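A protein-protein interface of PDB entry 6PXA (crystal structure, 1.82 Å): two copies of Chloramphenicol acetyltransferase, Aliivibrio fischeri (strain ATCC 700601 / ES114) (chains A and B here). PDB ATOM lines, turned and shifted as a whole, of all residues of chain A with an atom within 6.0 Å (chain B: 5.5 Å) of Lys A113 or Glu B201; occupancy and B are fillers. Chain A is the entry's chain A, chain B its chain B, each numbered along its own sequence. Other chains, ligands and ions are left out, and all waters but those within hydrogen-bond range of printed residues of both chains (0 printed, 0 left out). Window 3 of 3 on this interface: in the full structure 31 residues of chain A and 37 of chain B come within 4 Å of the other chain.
Among the printed residues, merely in contact across the chains: Trp A97 with Ser B205, Gly A111 with Met B200, Val A112 with Met B200, Trp A97 with Cys B204, Gly A111 with Glu B201 and Trp A97 with Leu B203.
No position is printed for both chains. Of the 8 pairs that touch across the chains among the printed residues, none has its exchanged pair printed and touching as well.
The side-chain amino group (NZ) of Lys A113 is in salt-bridge range of the side-chain carboxylate (OE2) of Glu B201, 3.4 Å away. N of Lys A113 lies within hydrogen-bond range of SG of Cys B204, 3.5 Å away.
Lys A113 touches two residues of chain B. Of the printed residues of chain A, Glu B201 touches Gly A111 (3.6 Å) and Lys A113 (3.4 Å). Of the printed residues of chain B, Trp A97 touches Leu B203, Cys B204 and Ser B205. Of the printed residues of chain A, Leu B203 touches Trp A97. Asn B198 touches none of the printed residues of chain A. The nearest residue of chain B that does not touch Lys A113 is Met B200 (5.2 Å). The nearest printed residue of chain B that does not touch Val A112 is Cys B204 (4.3 Å).
Printed residues of chain B that touch a printed residue of chain A: Met B200, Glu B201, Leu B203, Cys B204 and Ser B205. Hydrophobic or aromatic side chains of chain B within 4 Å of the printed part of chain A: Met B200.
O of Met B200 lies close to SG of Cys B204, at 3.7 Å. The backbone carbonyl oxygen (O) of Ile B202 is in hydrogen-bond range of the side-chain hydroxyl (OG) of Ser B205 (2.6 Å).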
ATOM      1  N   TRP A  97      18.025   9.745  15.080  1.00  0.00           N
ATOM      2  CA  TRP A  97      18.629   8.534  15.596  1.00  0.00           C
ATOM      3  C   TRP A  97      18.225   8.351  17.058  1.00  0.00           C
ATOM      4  O   TRP A  97      17.750   9.282  17.717  1.00  0.00           O
ATOM      5  CB  TRP A  97      20.148   8.607  15.451  1.00  0.00           C
ATOM      6  CG  TRP A  97      20.641   8.385  14.048  1.00  0.00           C
ATOM      7  CD1 TRP A  97      19.891   8.116  12.939  1.00  0.00           C
ATOM      8  CD2 TRP A  97      22.003   8.398  13.619  1.00  0.00           C
ATOM      9  NE1 TRP A  97      20.710   7.944  11.841  1.00  0.00           N
ATOM     10  CE2 TRP A  97      22.012   8.117  12.236  1.00  0.00           C
ATOM     11  CE3 TRP A  97      23.221   8.601  14.276  1.00  0.00           C
ATOM     12  CZ2 TRP A  97      23.190   8.031  11.506  1.00  0.00           C
ATOM     13  CZ3 TRP A  97      24.382   8.538  13.550  1.00  0.00           C
ATOM     14  CH2 TRP A  97      24.364   8.252  12.177  1.00  0.00           C
ATOM     15  N   LYS A 105      34.692   6.762  18.659  1.00  0.00           N
ATOM     16  CA  LYS A 105      35.156   5.425  18.317  1.00  0.00           C
ATOM     17  C   LYS A 105      36.117   4.889  19.374  1.00  0.00           C
ATOM     18  O   LYS A 105      36.014   3.723  19.785  1.00  0.00           O
ATOM     19  CB  LYS A 105      35.808   5.446  16.938  1.00  0.00           C
ATOM     20  CG  LYS A 105      35.134   4.525  15.917  1.00  0.00           C
ATOM     21  CD  LYS A 105      34.587   5.304  14.728  1.00  0.00           C
ATOM     22  CE  LYS A 105      33.702   4.434  13.840  1.00  0.00           C
ATOM     23  NZ  LYS A 105      34.449   3.298  13.218  1.00  0.00           N
ATOM     24  N   GLU A 110      33.801   0.168  16.915  1.00  0.00           N
ATOM     25  CA  GLU A 110      33.620   0.410  15.489  1.00  0.00           C
ATOM     26  C   GLU A 110      32.160   0.484  15.054  1.00  0.00           C
ATOM     27  O   GLU A 110      31.895   0.915  13.935  1.00  0.00           O
ATOM     28  CB  GLU A 110      34.358  -0.668  14.686  1.00  0.00           C
ATOM     29  CG  GLU A 110      35.636  -0.163  13.999  1.00  0.00           C
ATOM     30  CD  GLU A 110      36.746   0.219  14.974  1.00  0.00           C
ATOM     31  OE1 GLU A 110      36.563   1.160  15.774  1.00  0.00           O
ATOM     32  OE2 GLU A 110      37.816  -0.425  14.938  1.00  0.00           O
ATOM     33  N   GLY A 111      31.202   0.105  15.895  1.00  0.00           N
ATOM     34  CA  GLY A 111      29.816   0.277  15.494  1.00  0.00           C
ATOM     35  C   GLY A 111      29.367   1.724  15.404  1.00  0.00           C
ATOM     36  O   GLY A 111      28.236   1.972  14.967  1.00  0.00           O
ATOM     37  N   VAL A 112      30.225   2.672  15.796  1.00  0.00           N
ATOM     38  CA  VAL A 112      29.878   4.091  15.767  1.00  0.00           C
ATOM     39  C   VAL A 112      29.717   4.551  14.326  1.00  0.00           C
ATOM     40  O   VAL A 112      30.543   4.235  13.461  1.00  0.00           O
ATOM     41  CB  VAL A 112      30.948   4.927  16.486  1.00  0.00           C
ATOM     42  CG1 VAL A 112      30.572   6.393  16.465  1.00  0.00           C
ATOM     43  CG2 VAL A 112      31.138   4.445  17.918  1.00  0.00           C
ATOM     44  N   LYS A 113      28.633   5.268  14.061  1.00  0.00           N
ATOM     45  CA  LYS A 113      28.375   5.891  12.767  1.00  0.00           C
ATOM     46  C   LYS A 113      28.385   7.403  12.909  1.00  0.00           C
ATOM     47  O   LYS A 113      27.804   7.955  13.853  1.00  0.00           O
ATOM     48  CB  LYS A 113      27.029   5.438  12.188  1.00  0.00           C
ATOM     49  CG  LYS A 113      26.876   3.915  12.135  1.00  0.00           C
ATOM     50  CD  LYS A 113      25.634   3.495  11.349  1.00  0.00           C
ATOM     51  CE  LYS A 113      25.718   2.042  10.905  1.00  0.00           C
ATOM     52  NZ  LYS A 113      24.549   1.632  10.072  1.00  0.00           N
ATOM     53  N   ASP A 114      29.026   8.067  11.951  1.00  0.00           N
ATOM     54  CA  ASP A 114      29.135   9.520  11.945  1.00  0.00           C
ATOM     55  C   ASP A 114      27.776  10.150  11.644  1.00  0.00           C
ATOM     56  O   ASP A 114      27.236   9.977  10.543  1.00  0.00           O
ATOM     57  CB  ASP A 114      30.181   9.942  10.905  1.00  0.00           C
ATOM     58  CG  ASP A 114      30.392  11.462  10.835  1.00  0.00           C
ATOM     59  OD1 ASP A 114      29.831  12.212  11.660  1.00  0.00           O
ATOM     60  OD2 ASP A 114      31.128  11.913   9.933  1.00  0.00           O
ATOM     61  N   GLY A 115      27.235  10.900  12.609  1.00  0.00           N
ATOM     62  CA  GLY A 115      25.932  11.497  12.439  1.00  0.00           C
ATOM     63  C   GLY A 115      25.906  12.888  11.829  1.00  0.00           C
ATOM     64  O   GLY A 115      24.825  13.465  11.701  1.00  0.00           O
ATOM     65  N   LYS B 197      28.156  -0.831  23.538  1.00  0.00           N
ATOM     66  CA  LYS B 197      29.079  -1.042  22.433  1.00  0.00           C
ATOM     67  C   LYS B 197      28.493  -2.006  21.407  1.00  0.00           C
ATOM     68  O   LYS B 197      28.470  -1.706  20.206  1.00  0.00           O
ATOM     69  CB  LYS B 197      30.419  -1.542  22.972  1.00  0.00           C
ATOM     70  CG  LYS B 197      31.083  -0.530  23.893  1.00  0.00           C
ATOM     71  CD  LYS B 197      32.463  -0.984  24.334  1.00  0.00           C
ATOM     72  CE  LYS B 197      33.410  -1.094  23.157  1.00  0.00           C
ATOM     73  NZ  LYS B 197      34.810  -1.346  23.592  1.00  0.00           N
ATOM     74  N   ASN B 198      27.969  -3.151  21.872  1.00  0.00           N
ATOM     75  CA  ASN B 198      27.461  -4.174  20.957  1.00  0.00           C
ATOM     76  C   ASN B 198      26.311  -3.662  20.108  1.00  0.00           C
ATOM     77  O   ASN B 198      26.114  -4.131  18.982  1.00  0.00           O
ATOM     78  CB  ASN B 198      26.987  -5.416  21.720  1.00  0.00           C
ATOM     79  CG  ASN B 198      28.126  -6.223  22.294  1.00  0.00           C
ATOM     80  OD1 ASN B 198      29.286  -5.999  21.956  1.00  0.00           O
ATOM     81  ND2 ASN B 198      27.800  -7.176  23.160  1.00  0.00           N
ATOM     82  N   THR B 199      25.518  -2.733  20.630  1.00  0.00           N
ATOM     83  CA  THR B 199      24.357  -2.261  19.895  1.00  0.00           C
ATOM     84  C   THR B 199      24.590  -0.890  19.279  1.00  0.00           C
ATOM     85  O   THR B 199      23.638  -0.260  18.810  1.00  0.00           O
ATOM     86  CB  THR B 199      23.137  -2.252  20.807  1.00  0.00           C
ATOM     87  OG1 THR B 199      23.268  -3.314  21.757  1.00  0.00           O
ATOM     88  CG2 THR B 199      21.903  -2.519  19.997  1.00  0.00           C
ATOM     89  N   MET B 200      25.842  -0.433  19.251  1.00  0.00           N
ATOM     90  CA  MET B 200      26.148   0.895  18.739  1.00  0.00           C
ATOM     91  C   MET B 200      25.634   1.104  17.313  1.00  0.00           C
ATOM     92  O   MET B 200      25.230   2.219  16.958  1.00  0.00           O
ATOM     93  CB  MET B 200      27.653   1.135  18.821  1.00  0.00           C
ATOM     94  CG  MET B 200      28.061   2.535  18.420  1.00  0.00           C
ATOM     95  SD  MET B 200      27.190   3.804  19.358  1.00  0.00           S
ATOM     96  CE  MET B 200      27.665   3.322  21.022  1.00  0.00           C
ATOM     97  N   GLU B 201      25.637   0.055  16.486  1.00  0.00           N
ATOM     98  CA  GLU B 201      25.086   0.163  15.140  1.00  0.00           C
ATOM     99  C   GLU B 201      23.598   0.484  15.171  1.00  0.00           C
ATOM    100  O   GLU B 201      23.097   1.187  14.285  1.00  0.00           O
ATOM    101  CB  GLU B 201      25.337  -1.134  14.368  1.00  0.00           C
ATOM    102  CG  GLU B 201      25.709  -0.942  12.909  1.00  0.00           C
ATOM    103  CD  GLU B 201      24.548  -1.200  11.959  1.00  0.00           C
ATOM    104  OE1 GLU B 201      23.390  -0.933  12.350  1.00  0.00           O
ATOM    105  OE2 GLU B 201      24.794  -1.675  10.825  1.00  0.00           O
ATOM    106  N   ILE B 202      22.876  -0.010  16.175  1.00  0.00           N
ATOM    107  CA  ILE B 202      21.456   0.312  16.274  1.00  0.00           C
ATOM    108  C   ILE B 202      21.244   1.704  16.867  1.00  0.00           C
ATOM    109  O   ILE B 202      20.357   2.438  16.422  1.00  0.00           O
ATOM    110  CB  ILE B 202      20.703  -0.761  17.083  1.00  0.00           C
ATOM    111  CG1 ILE B 202      20.913  -2.151  16.479  1.00  0.00           C
ATOM    112  CG2 ILE B 202      19.214  -0.444  17.122  1.00  0.00           C
ATOM    113  CD1 ILE B 202      20.078  -3.240  17.160  1.00  0.00           C
ATOM    114  N   LEU B 203      22.032   2.091  17.882  1.00  0.00           N
ATOM    115  CA  LEU B 203      21.864   3.421  18.477  1.00  0.00           C
ATOM    116  C   LEU B 203      22.176   4.545  17.478  1.00  0.00           C
ATOM    117  O   LEU B 203      21.579   5.627  17.551  1.00  0.00           O
ATOM    118  CB  LEU B 203      22.743   3.563  19.725  1.00  0.00           C
ATOM    119  CG  LEU B 203      22.463   2.654  20.943  1.00  0.00           C
ATOM    120  CD1 LEU B 203      23.639   2.656  21.904  1.00  0.00           C
ATOM    121  CD2 LEU B 203      21.201   3.071  21.663  1.00  0.00           C
ATOM    122  N   CYS B 204      23.095   4.314  16.548  1.00  0.00           N
ATOM    123  CA  CYS B 204      23.350   5.242  15.444  1.00  0.00           C
ATOM    124  C   CYS B 204      22.398   4.984  14.280  1.00  0.00           C
ATOM    125  O   CYS B 204      22.809   4.820  13.138  1.00  0.00           O
ATOM    126  CB  CYS B 204      24.804   5.150  14.993  1.00  0.00           C
ATOM    127  SG  CYS B 204      25.985   5.741  16.255  1.00  0.00           S
ATOM    128  N   SER B 205      21.105   4.965  14.590  1.00  0.00           N
ATOM    129  CA  SER B 205      20.042   4.725  13.625  1.00  0.00           C
ATOM    130  C   SER B 205      18.724   5.008  14.326  1.00  0.00           C
ATOM    131  O   SER B 205      18.680   5.271  15.534  1.00  0.00           O
ATOM    132  CB  SER B 205      20.057   3.295  13.085  1.00  0.00           C
ATOM    133  OG  SER B 205      19.429   2.417  14.005  1.00  0.00           O
